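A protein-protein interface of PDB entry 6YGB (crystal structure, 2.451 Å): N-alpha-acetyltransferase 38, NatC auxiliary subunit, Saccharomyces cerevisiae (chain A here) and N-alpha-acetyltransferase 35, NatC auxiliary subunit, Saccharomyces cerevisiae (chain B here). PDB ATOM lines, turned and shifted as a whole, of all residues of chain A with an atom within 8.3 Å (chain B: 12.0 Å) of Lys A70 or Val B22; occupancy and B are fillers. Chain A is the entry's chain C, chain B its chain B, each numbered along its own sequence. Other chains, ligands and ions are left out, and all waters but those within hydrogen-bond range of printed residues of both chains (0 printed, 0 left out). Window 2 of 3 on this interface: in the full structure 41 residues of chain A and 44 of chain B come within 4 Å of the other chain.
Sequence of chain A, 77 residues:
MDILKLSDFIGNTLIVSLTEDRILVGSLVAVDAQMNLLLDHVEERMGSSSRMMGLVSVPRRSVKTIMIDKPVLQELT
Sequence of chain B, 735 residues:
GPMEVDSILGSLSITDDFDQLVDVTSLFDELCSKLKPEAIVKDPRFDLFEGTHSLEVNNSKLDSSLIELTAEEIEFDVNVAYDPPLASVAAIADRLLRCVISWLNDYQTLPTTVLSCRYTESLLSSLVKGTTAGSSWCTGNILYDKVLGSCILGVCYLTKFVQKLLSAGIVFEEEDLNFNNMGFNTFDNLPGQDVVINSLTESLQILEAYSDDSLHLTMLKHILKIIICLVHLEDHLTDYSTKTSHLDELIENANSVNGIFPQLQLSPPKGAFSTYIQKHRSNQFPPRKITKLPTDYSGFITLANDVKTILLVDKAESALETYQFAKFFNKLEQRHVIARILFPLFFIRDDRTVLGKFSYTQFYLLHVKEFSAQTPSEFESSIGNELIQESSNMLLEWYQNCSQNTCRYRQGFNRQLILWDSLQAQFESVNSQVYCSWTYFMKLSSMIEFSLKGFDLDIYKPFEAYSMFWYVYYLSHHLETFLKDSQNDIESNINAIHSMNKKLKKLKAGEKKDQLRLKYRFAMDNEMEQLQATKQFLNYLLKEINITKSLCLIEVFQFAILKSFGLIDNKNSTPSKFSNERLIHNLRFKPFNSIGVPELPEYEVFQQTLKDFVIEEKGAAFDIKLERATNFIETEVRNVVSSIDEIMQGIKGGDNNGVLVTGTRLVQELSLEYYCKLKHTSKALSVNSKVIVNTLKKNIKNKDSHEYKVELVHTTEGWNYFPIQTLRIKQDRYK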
ATOM      1  N   PHE A   9      10.649  27.467  -6.150  1.00  0.00           N
ATOM      2  CA  PHE A   9      11.366  26.710  -7.167  1.00  0.00           C
ATOM      3  C   PHE A   9      11.688  25.290  -6.724  1.00  0.00           C
ATOM      4  O   PHE A   9      11.905  24.426  -7.582  1.00  0.00           O
ATOM      5  CB  PHE A   9      12.665  27.425  -7.550  1.00  0.00           C
ATOM      6  CG  PHE A   9      12.470  28.592  -8.474  1.00  0.00           C
ATOM      7  CD1 PHE A   9      12.450  28.409  -9.849  1.00  0.00           C
ATOM      8  CD2 PHE A   9      12.321  29.874  -7.971  1.00  0.00           C
ATOM      9  CE1 PHE A   9      12.276  29.482 -10.701  1.00  0.00           C
ATOM     10  CE2 PHE A   9      12.147  30.949  -8.820  1.00  0.00           C
ATOM     11  CZ  PHE A   9      12.124  30.752 -10.184  1.00  0.00           C
ATOM     12  N   LEU A  14      14.425  22.030 -13.608  1.00  0.00           N
ATOM     13  CA  LEU A  14      15.201  23.147 -14.119  1.00  0.00           C
ATOM     14  C   LEU A  14      16.053  22.679 -15.287  1.00  0.00           C
ATOM     15  O   LEU A  14      16.394  21.498 -15.390  1.00  0.00           O
ATOM     16  CB  LEU A  14      16.102  23.745 -13.034  1.00  0.00           C
ATOM     17  CG  LEU A  14      15.421  24.304 -11.787  1.00  0.00           C
ATOM     18  CD1 LEU A  14      16.437  24.967 -10.872  1.00  0.00           C
ATOM     19  CD2 LEU A  14      14.314  25.283 -12.159  1.00  0.00           C
ATOM     20  N   ILE A  15      16.387  23.611 -16.170  1.00  0.00           N
ATOM     21  CA  ILE A  15      17.284  23.353 -17.288  1.00  0.00           C
ATOM     22  C   ILE A  15      18.557  24.134 -17.011  1.00  0.00           C
ATOM     23  O   ILE A  15      18.556  25.371 -17.042  1.00  0.00           O
ATOM     24  CB  ILE A  15      16.669  23.748 -18.638  1.00  0.00           C
ATOM     25  CG1 ILE A  15      15.521  22.805 -19.007  1.00  0.00           C
ATOM     26  CG2 ILE A  15      17.730  23.745 -19.735  1.00  0.00           C
ATOM     27  CD1 ILE A  15      14.196  23.150 -18.350  1.00  0.00           C
ATOM     28  N   THR A  65      24.010  28.768 -17.000  1.00  0.00           N
ATOM     29  CA  THR A  65      22.707  29.411 -16.955  1.00  0.00           C
ATOM     30  C   THR A  65      21.679  28.441 -16.393  1.00  0.00           C
ATOM     31  O   THR A  65      21.850  27.220 -16.444  1.00  0.00           O
ATOM     32  CB  THR A  65      22.270  29.899 -18.341  1.00  0.00           C
ATOM     33  OG1 THR A  65      21.016  30.581 -18.232  1.00  0.00           O
ATOM     34  CG2 THR A  65      22.109  28.727 -19.287  1.00  0.00           C
ATOM     35  N   ILE A  66      20.603  29.010 -15.860  1.00  0.00           N
ATOM     36  CA  ILE A  66      19.491  28.248 -15.302  1.00  0.00           C
ATOM     37  C   ILE A  66      18.209  28.717 -15.976  1.00  0.00           C
ATOM     38  O   ILE A  66      17.930  29.919 -16.017  1.00  0.00           O
ATOM     39  CB  ILE A  66      19.387  28.422 -13.775  1.00  0.00           C
ATOM     40  CG1 ILE A  66      20.754  28.207 -13.117  1.00  0.00           C
ATOM     41  CG2 ILE A  66      18.353  27.468 -13.200  1.00  0.00           C
ATOM     42  CD1 ILE A  66      20.776  28.557 -11.644  1.00  0.00           C
ATOM     43  N   MET A  67      17.426  27.772 -16.495  1.00  0.00           N
ATOM     44  CA  MET A  67      16.201  28.086 -17.218  1.00  0.00           C
ATOM     45  C   MET A  67      15.065  27.183 -16.762  1.00  0.00           C
ATOM     46  O   MET A  67      15.275  26.000 -16.479  1.00  0.00           O
ATOM     47  CB  MET A  67      16.402  27.942 -18.732  1.00  0.00           C
ATOM     48  CG  MET A  67      17.349  28.966 -19.333  1.00  0.00           C
ATOM     49  SD  MET A  67      17.465  28.829 -21.125  1.00  0.00           S
ATOM     50  CE  MET A  67      18.453  30.277 -21.507  1.00  0.00           C
ATOM     51  N   ILE A  68      13.859  27.745 -16.703  1.00  0.00           N
ATOM     52  CA  ILE A  68      12.658  27.013 -16.316  1.00  0.00           C
ATOM     53  C   ILE A  68      11.597  27.201 -17.393  1.00  0.00           C
ATOM     54  O   ILE A  68      11.496  28.274 -18.000  1.00  0.00           O
ATOM     55  CB  ILE A  68      12.129  27.463 -14.936  1.00  0.00           C
ATOM     56  CG1 ILE A  68      10.986  26.558 -14.477  1.00  0.00           C
ATOM     57  CG2 ILE A  68      11.663  28.913 -14.968  1.00  0.00           C
ATOM     58  CD1 ILE A  68      10.313  27.024 -13.208  1.00  0.00           C
ATOM     59  N   ASP A  69      10.815  26.150 -17.636  1.00  0.00           N
ATOM     60  CA  ASP A  69       9.734  26.225 -18.608  1.00  0.00           C
ATOM     61  C   ASP A  69       8.710  27.261 -18.163  1.00  0.00           C
ATOM     62  O   ASP A  69       8.372  27.345 -16.979  1.00  0.00           O
ATOM     63  CB  ASP A  69       9.081  24.852 -18.774  1.00  0.00           C
ATOM     64  CG  ASP A  69       8.582  24.607 -20.186  1.00  0.00           C
ATOM     65  OD1 ASP A  69       9.418  24.358 -21.077  1.00  0.00           O
ATOM     66  OD2 ASP A  69       7.353  24.642 -20.403  1.00  0.00           O
ATOM     67  N   LYS A  70       8.234  28.064 -19.116  1.00  0.00           N
ATOM     68  CA  LYS A  70       7.321  29.152 -18.773  1.00  0.00           C
ATOM     69  C   LYS A  70       6.031  28.671 -18.119  1.00  0.00           C
ATOM     70  O   LYS A  70       5.595  29.301 -17.138  1.00  0.00           O
ATOM     71  CB  LYS A  70       7.033  29.990 -20.022  1.00  0.00           C
ATOM     72  CG  LYS A  70       6.131  31.192 -19.770  1.00  0.00           C
ATOM     73  CD  LYS A  70       5.649  31.772 -21.090  1.00  0.00           C
ATOM     74  CE  LYS A  70       5.110  33.181 -20.932  1.00  0.00           C
ATOM     75  NZ  LYS A  70       6.164  34.112 -20.443  1.00  0.00           N
ATOM     76  N   PRO A  71       5.362  27.611 -18.611  1.00  0.00           N
ATOM     77  CA  PRO A  71       4.160  27.102 -17.918  1.00  0.00           C
ATOM     78  C   PRO A  71       4.346  26.885 -16.425  1.00  0.00           C
ATOM     79  O   PRO A  71       3.559  27.404 -15.624  1.00  0.00           O
ATOM     80  CB  PRO A  71       3.864  25.791 -18.669  1.00  0.00           C
ATOM     81  CG  PRO A  71       4.326  26.062 -20.072  1.00  0.00           C
ATOM     82  CD  PRO A  71       5.542  26.966 -19.924  1.00  0.00           C
ATOM     83  N   VAL A  72       5.393  26.162 -16.023  1.00  0.00           N
ATOM     84  CA  VAL A  72       5.603  25.894 -14.599  1.00  0.00           C
ATOM     85  C   VAL A  72       5.877  27.188 -13.843  1.00  0.00           C
ATOM     86  O   VAL A  72       5.448  27.356 -12.694  1.00  0.00           O
ATOM     87  CB  VAL A  72       6.741  24.876 -14.395  1.00  0.00           C
ATOM     88  CG1 VAL A  72       6.745  24.363 -12.957  1.00  0.00           C
ATOM     89  CG2 VAL A  72       6.604  23.730 -15.379  1.00  0.00           C
ATOM     90  N   LEU A  73       6.584  28.126 -14.479  1.00  0.00           N
ATOM     91  CA  LEU A  73       6.932  29.381 -13.819  1.00  0.00           C
ATOM     92  C   LEU A  73       5.692  30.192 -13.460  1.00  0.00           C
ATOM     93  O   LEU A  73       5.646  30.836 -12.406  1.00  0.00           O
ATOM     94  CB  LEU A  73       7.868  30.193 -14.718  1.00  0.00           C
ATOM     95  CG  LEU A  73       8.279  31.588 -14.242  1.00  0.00           C
ATOM     96  CD1 LEU A  73       8.983  31.504 -12.900  1.00  0.00           C
ATOM     97  CD2 LEU A  73       9.162  32.272 -15.276  1.00  0.00           C
ATOM     98  N   GLN A  74       4.672  30.170 -14.320  1.00  0.00           N
ATOM     99  CA  GLN A  74       3.476  30.957 -14.045  1.00  0.00           C
ATOM    100  C   GLN A  74       2.614  30.316 -12.964  1.00  0.00           C
ATOM    101  O   GLN A  74       1.836  31.013 -12.302  1.00  0.00           O
ATOM    102  CB  GLN A  74       2.668  31.160 -15.329  1.00  0.00           C
ATOM    103  CG  GLN A  74       3.489  31.646 -16.520  1.00  0.00           C
ATOM    104  CD  GLN A  74       4.333  32.874 -16.214  1.00  0.00           C
ATOM    105  OE1 GLN A  74       3.952  33.727 -15.411  1.00  0.00           O
ATOM    106  NE2 GLN A  74       5.489  32.968 -16.861  1.00  0.00           N
ATOM    107  N   GLU A  75       2.736  29.001 -12.767  1.00  0.00           N
ATOM    108  CA  GLU A  75       1.994  28.347 -11.694  1.00  0.00           C
ATOM    109  C   GLU A  75       2.559  28.719 -10.327  1.00  0.00           C
ATOM    110  O   GLU A  75       1.801  28.972  -9.385  1.00  0.00           O
ATOM    111  CB  GLU A  75       2.011  26.828 -11.890  1.00  0.00           C
ATOM    112  CG  GLU A  75       0.976  26.067 -11.059  1.00  0.00           C
ATOM    113  CD  GLU A  75       1.349  25.951  -9.588  1.00  0.00           C
ATOM    114  OE1 GLU A  75       2.556  25.868  -9.275  1.00  0.00           O
ATOM    115  OE2 GLU A  75       0.431  25.950  -8.742  1.00  0.00           O
ATOM    116  N   LEU A  76       3.890  28.767 -10.206  1.00  0.00           N
ATOM    117  CA  LEU A  76       4.527  29.022  -8.917  1.00  0.00           C
ATOM    118  C   LEU A  76       4.164  30.393  -8.362  1.00  0.00           C
ATOM    119  O   LEU A  76       4.134  30.582  -7.140  1.00  0.00           O
ATOM    120  CB  LEU A  76       6.044  28.893  -9.052  1.00  0.00           C
ATOM    121  CG  LEU A  76       6.560  27.629  -9.741  1.00  0.00           C
ATOM    122  CD1 LEU A  76       8.083  27.595  -9.743  1.00  0.00           C
ATOM    123  CD2 LEU A  76       5.983  26.392  -9.072  1.00  0.00           C
ATOM    124  N   THR A  77       3.872  31.351  -9.237  1.00  0.00           N
ATOM    125  CA  THR A  77       3.528  32.704  -8.820  1.00  0.00           C
ATOM    126  C   THR A  77       2.173  32.723  -8.097  1.00  0.00           C
ATOM    127  O   THR A  77       1.617  33.774  -7.766  1.00  0.00           O
ATOM    128  CB  THR A  77       3.504  33.668 -10.032  1.00  0.00           C
ATOM    129  OG1 THR A  77       4.626  33.394 -10.882  1.00  0.00           O
ATOM    130  CG2 THR A  77       3.579  35.120  -9.573  1.00  0.00           C
ATOM    131  OXT THR A  77       1.601  31.667  -7.814  1.00  0.00           O
ATOM    132  N   THR B  15      16.373  21.353 -26.739  1.00  0.00           N
ATOM    133  CA  THR B  15      15.298  22.004 -26.005  1.00  0.00           C
ATOM    134  C   THR B  15      13.942  21.862 -26.686  1.00  0.00           C
ATOM    135  O   THR B  15      12.998  22.562 -26.306  1.00  0.00           O
ATOM    136  CB  THR B  15      15.618  23.489 -25.806  1.00  0.00           C
ATOM    137  OG1 THR B  15      15.816  24.113 -27.082  1.00  0.00           O
ATOM    138  CG2 THR B  15      16.876  23.658 -24.963  1.00  0.00           C
ATOM    139  N   ASP B  16      13.824  20.973 -27.676  1.00  0.00           N
ATOM    140  CA  ASP B  16      12.570  20.848 -28.416  1.00  0.00           C
ATOM    141  C   ASP B  16      11.448  20.318 -27.534  1.00  0.00           C
ATOM    142  O   ASP B  16      10.292  20.735 -27.678  1.00  0.00           O
ATOM    143  CB  ASP B  16      12.761  19.945 -29.633  1.00  0.00           C
ATOM    144  CG  ASP B  16      13.319  20.691 -30.831  1.00  0.00           C
ATOM    145  OD1 ASP B  16      13.639  21.889 -30.694  1.00  0.00           O
ATOM    146  OD2 ASP B  16      13.432  20.077 -31.916  1.00  0.00           O
ATOM    147  N   ASP B  17      11.764  19.394 -26.623  1.00  0.00           N
ATOM    148  CA  ASP B  17      10.747  18.848 -25.730  1.00  0.00           C
ATOM    149  C   ASP B  17      10.107  19.919 -24.857  1.00  0.00           C
ATOM    150  O   ASP B  17       9.037  19.682 -24.287  1.00  0.00           O
ATOM    151  CB  ASP B  17      11.353  17.750 -24.853  1.00  0.00           C
ATOM    152  CG  ASP B  17      12.715  18.126 -24.306  1.00  0.00           C
ATOM    153  OD1 ASP B  17      13.387  18.982 -24.918  1.00  0.00           O
ATOM    154  OD2 ASP B  17      13.121  17.560 -23.269  1.00  0.00           O
ATOM    155  N   PHE B  18      10.730  21.086 -24.742  1.00  0.00           N
ATOM    156  CA  PHE B  18      10.177  22.199 -23.985  1.00  0.00           C
ATOM    157  C   PHE B  18       9.519  23.192 -24.934  1.00  0.00           C
ATOM    158  O   PHE B  18      10.120  23.593 -25.937  1.00  0.00           O
ATOM    159  CB  PHE B  18      11.267  22.888 -23.165  1.00  0.00           C
ATOM    160  CG  PHE B  18      11.865  22.012 -22.103  1.00  0.00           C
ATOM    161  CD1 PHE B  18      11.223  21.836 -20.887  1.00  0.00           C
ATOM    162  CD2 PHE B  18      13.068  21.360 -22.319  1.00  0.00           C
ATOM    163  CE1 PHE B  18      11.770  21.025 -19.903  1.00  0.00           C
ATOM    164  CE2 PHE B  18      13.620  20.549 -21.343  1.00  0.00           C
ATOM    165  CZ  PHE B  18      12.970  20.380 -20.134  1.00  0.00           C
ATOM    166  N   ASP B  19       8.283  23.585 -24.616  1.00  0.00           N
ATOM    167  CA  ASP B  19       7.586  24.567 -25.441  1.00  0.00           C
ATOM    168  C   ASP B  19       8.226  25.944 -25.322  1.00  0.00           C
ATOM    169  O   ASP B  19       8.392  26.647 -26.327  1.00  0.00           O
ATOM    170  CB  ASP B  19       6.111  24.630 -25.045  1.00  0.00           C
ATOM    171  CG  ASP B  19       5.338  25.665 -25.839  1.00  0.00           C
ATOM    172  OD1 ASP B  19       5.715  25.935 -27.000  1.00  0.00           O
ATOM    173  OD2 ASP B  19       4.355  26.215 -25.297  1.00  0.00           O
ATOM    174  N   GLN B  20       8.592  26.347 -24.106  1.00  0.00           N
ATOM    175  CA  GLN B  20       9.142  27.674 -23.874  1.00  0.00           C
ATOM    176  C   GLN B  20      10.132  27.628 -22.719  1.00  0.00           C
ATOM    177  O   GLN B  20       9.924  26.906 -21.743  1.00  0.00           O
ATOM    178  CB  GLN B  20       8.024  28.681 -23.579  1.00  0.00           C
ATOM    179  CG  GLN B  20       8.462  30.134 -23.579  1.00  0.00           C
ATOM    180  CD  GLN B  20       8.635  30.694 -24.975  1.00  0.00           C
ATOM    181  OE1 GLN B  20       9.044  29.990 -25.897  1.00  0.00           O
ATOM    182  NE2 GLN B  20       8.313  31.971 -25.141  1.00  0.00           N
ATOM    183  N   LEU B  21      11.208  28.404 -22.834  1.00  0.00           N
ATOM    184  CA  LEU B  21      12.226  28.468 -21.795  1.00  0.00           C
ATOM    185  C   LEU B  21      12.497  29.916 -21.419  1.00  0.00           C
ATOM    186  O   LEU B  21      12.577  30.790 -22.285  1.00  0.00           O
ATOM    187  CB  LEU B  21      13.531  27.797 -22.243  1.00  0.00           C
ATOM    188  CG  LEU B  21      13.545  26.268 -22.273  1.00  0.00           C
ATOM    189  CD1 LEU B  21      14.922  25.752 -22.660  1.00  0.00           C
ATOM    190  CD2 LEU B  21      13.118  25.700 -20.928  1.00  0.00           C
ATOM    191  N   VAL B  22      12.647  30.163 -20.120  1.00  0.00           N
ATOM    192  CA  VAL B  22      12.921  31.495 -19.594  1.00  0.00           C
ATOM    193  C   VAL B  22      14.199  31.435 -18.769  1.00  0.00           C
ATOM    194  O   VAL B  22      14.320  30.601 -17.866  1.00  0.00           O
ATOM    195  CB  VAL B  22      11.754  32.022 -18.740  1.00  0.00           C
ATOM    196  CG1 VAL B  22      11.991  33.476 -18.364  1.00  0.00           C
ATOM    197  CG2 VAL B  22      10.432  31.858 -19.475  1.00  0.00           C
ATOM    198  N   ASP B  23      15.144  32.323 -19.071  1.00  0.00           N
ATOM    199  CA  ASP B  23      16.377  32.386 -18.298  1.00  0.00           C
ATOM    200  C   ASP B  23      16.089  32.965 -16.918  1.00  0.00           C
ATOM    201  O   ASP B  23      15.445  34.010 -16.790  1.00  0.00           O
ATOM    202  CB  ASP B  23      17.428  33.225 -19.027  1.00  0.00           C
ATOM    203  CG  ASP B  23      18.769  33.239 -18.312  1.00  0.00           C
ATOM    204  OD1 ASP B  23      18.878  32.660 -17.212  1.00  0.00           O
ATOM    205  OD2 ASP B  23      19.724  33.832 -18.854  1.00  0.00           O
ATOM    206  N   VAL B  24      16.568  32.274 -15.882  1.00  0.00           N
ATOM    207  CA  VAL B  24      16.352  32.644 -14.490  1.00  0.00           C
ATOM    208  C   VAL B  24      17.669  32.847 -13.750  1.00  0.00           C
ATOM    209  O   VAL B  24      17.676  33.010 -12.529  1.00  0.00           O
ATOM    210  CB  VAL B  24      15.477  31.596 -13.771  1.00  0.00           C
ATOM    211  CG1 VAL B  24      14.888  32.148 -12.481  1.00  0.00           C
ATOM    212  CG2 VAL B  24      14.367  31.134 -14.682  1.00  0.00           C
ATOM    213  N   THR B  25      18.790  32.841 -14.471  1.00  0.00           N
ATOM    214  CA  THR B  25      20.103  32.936 -13.840  1.00  0.00           C
ATOM    215  C   THR B  25      20.216  34.178 -12.966  1.00  0.00           C
ATOM    216  O   THR B  25      20.594  34.099 -11.792  1.00  0.00           O
ATOM    217  CB  THR B  25      21.194  32.938 -14.910  1.00  0.00           C
ATOM    218  OG1 THR B  25      20.952  31.870 -15.832  1.00  0.00           O
ATOM    219  CG2 THR B  25      22.562  32.746 -14.274  1.00  0.00           C
ATOM    220  N   SER B  26      19.889  35.342 -13.533  1.00  0.00           N
ATOM    221  CA  SER B  26      20.043  36.594 -12.800  1.00  0.00           C
ATOM    222  C   SER B  26      19.168  36.620 -11.553  1.00  0.00           C
ATOM    223  O   SER B  26      19.604  37.078 -10.491  1.00  0.00           O
ATOM    224  CB  SER B  26      19.719  37.777 -13.713  1.00  0.00           C
ATOM    225  OG  SER B  26      18.405  37.674 -14.231  1.00  0.00           O
ATOM    226  N   LEU B  27      17.933  36.120 -11.659  1.00  0.00           N
ATOM    227  CA  LEU B  27      17.034  36.095 -10.508  1.00  0.00           C
ATOM    228  C   LEU B  27      17.575  35.199  -9.398  1.00  0.00           C
ATOM    229  O   LEU B  27      17.524  35.558  -8.216  1.00  0.00           O
ATOM    230  CB  LEU B  27      15.642  35.628 -10.938  1.00  0.00           C
ATOM    231  CG  LEU B  27      14.702  35.167  -9.818  1.00  0.00           C
ATOM    232  CD1 LEU B  27      14.436  36.295  -8.830  1.00  0.00           C
ATOM    233  CD2 LEU B  27      13.394  34.630 -10.386  1.00  0.00           C
ATOM    234  N   PHE B  28      18.085  34.020  -9.763  1.00  0.00           N
ATOM    235  CA  PHE B  28      18.604  33.083  -8.768  1.00  0.00           C
ATOM    236  C   PHE B  28      19.739  33.704  -7.966  1.00  0.00           C
ATOM    237  O   PHE B  28      19.802  33.560  -6.740  1.00  0.00           O
ATOM    238  CB  PHE B  28      19.073  31.802  -9.458  1.00  0.00           C
ATOM    239  CG  PHE B  28      18.130  30.643  -9.301  1.00  0.00           C
ATOM    240  CD1 PHE B  28      16.844  30.699  -9.805  1.00  0.00           C
ATOM    241  CD2 PHE B  28      18.544  29.485  -8.666  1.00  0.00           C
ATOM    242  CE1 PHE B  28      15.983  29.627  -9.664  1.00  0.00           C
ATOM    243  CE2 PHE B  28      17.691  28.411  -8.523  1.00  0.00           C
ATOM    244  CZ  PHE B  28      16.409  28.481  -9.022  1.00  0.00           C
ATOM    245  N   ASP B  29      20.654  34.399  -8.647  1.00  0.00           N
ATOM    246  CA  ASP B  29      21.769  35.034  -7.951  1.00  0.00           C
ATOM    247  C   ASP B  29      21.279  36.107  -6.989  1.00  0.00           C
ATOM    248  O   ASP B  29      21.742  36.186  -5.844  1.00  0.00           O
ATOM    249  CB  ASP B  29      22.748  35.630  -8.964  1.00  0.00           C
ATOM    250  CG  ASP B  29      24.047  36.075  -8.326  1.00  0.00           C
ATOM    251  OD1 ASP B  29      24.215  35.866  -7.105  1.00  0.00           O
ATOM    252  OD2 ASP B  29      24.905  36.629  -9.045  1.00  0.00           O
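The side-chain carboxylate of Asp B23 lies within hydrogen-bond range of the side-chain hydroxyl of Thr B25. The backbone NH (N) of Ile A15 lies within hydrogen-bond range of the backbone carbonyl oxygen (O) of Met A67 (2.7 Å).
O of Gln B20 lies close to OD1 of Asp A69, at 2.7 Å. The backbone carbonyl oxygen of Gln B20 is in hydrogen-bond range of the backbone NH of Lys A70, 3.3 Å away. The backbone NH (N) of Val B22 is in hydrogen-bond range of the backbone carbonyl oxygen (O) of Ile A68 (3.1 Å). The side-chain carboxylate (OD1) of Asp B23 lies within hydrogen-bond range of the side-chain hydroxyl (OG1) of Thr A65 (3.2 Å). The backbone NH (N) of Val B24 lies within hydrogen-bond range of the backbone carbonyl oxygen (O) of Ile A66 (2.7 Å). OG1 of Thr A65 is in hydrogen-bond range of OG1 of Thr B25 (2.7 Å). The backbone NH of Ile A66 sits at hydrogen-bond distance from the side-chain hydroxyl of Thr B25, 2.9 Å away. The backbone carbonyl oxygen of Ile A66 sits close to the side-chain carboxylate of Asp B23, 3.1 Å away.
Among the printed residues, merely in contact across the chains: Phe A9 with Val B24, Phe A9 with Phe B28, Leu A14 with Phe B28, Ile A15 with Phe B18, Ile A15 with Leu B21, Ile A66 with Phe B28, Met A67 with Val B22, Met A67 with Asp B23, Ile A68 with Leu B21, Ile A68 with Val B24, Asp A69 with Phe B18, Asp A69 with Asp B19, Asp A69 with Leu B21 and Lys A70 with Val B22.
Of the printed residues of chain B, Phe A9 touches Val B24 (3.9 Å) and Phe B28 (3.7 Å). Printed residues of chain B within 4 Å of Leu A14: Phe B28 (3.97 Å). Printed residues of chain B within 4 Å of Thr A65: Asp B23 and Thr B25. Of chain B, only Leu B21, Val B22 and Val B24 come within 4 Å of Ile A68. Of the printed residues of chain B, Asp A69 touches Phe B18, Asp B19, Gln B20 and Leu B21. Lys A70 touches just these residues of chain B: Gln B20 and Val B22. No residue of chain B comes within 4 Å of Pro A71. No residue of chain B comes within 4 Å of Leu A73. Of the printed residues of chain A, Phe B18 touches Ile A15 and Asp A69. Val B22 touches just these residues of chain A: Met A67, Ile A68 and Lys A70. Of the printed residues of chain A, Val B24 touches Phe A9 (3.9 Å), Ile A66 (2.7 Å) and Ile A68 (3.5 Å). The nearest residue of chain A that does not touch Val B22 is Ile A66 (4.1 Å).
Of the 16 printed residues of chain A, 9 touch a printed residue of chain B. Printed residues of chain A that touch a printed residue of chain B: Phe A9, Leu A14, Ile A15, Thr A65, Ile A66, Met A67, Ile A68, Asp A69 and Lys A70. Hydrophobic or aromatic side chains of chain A within 4 Å of the printed part of chain B: Phe A9, Leu A14, Ile A15, Ile A66, Met A67 and Ile A68. Of the 15 printed residues of chain B, 9 touch a printed residue of chain A. Among the printed residues, no Asp or Glu carboxylate lies within 4 Å of a Lys or Arg side-chain nitrogen of the other chain.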
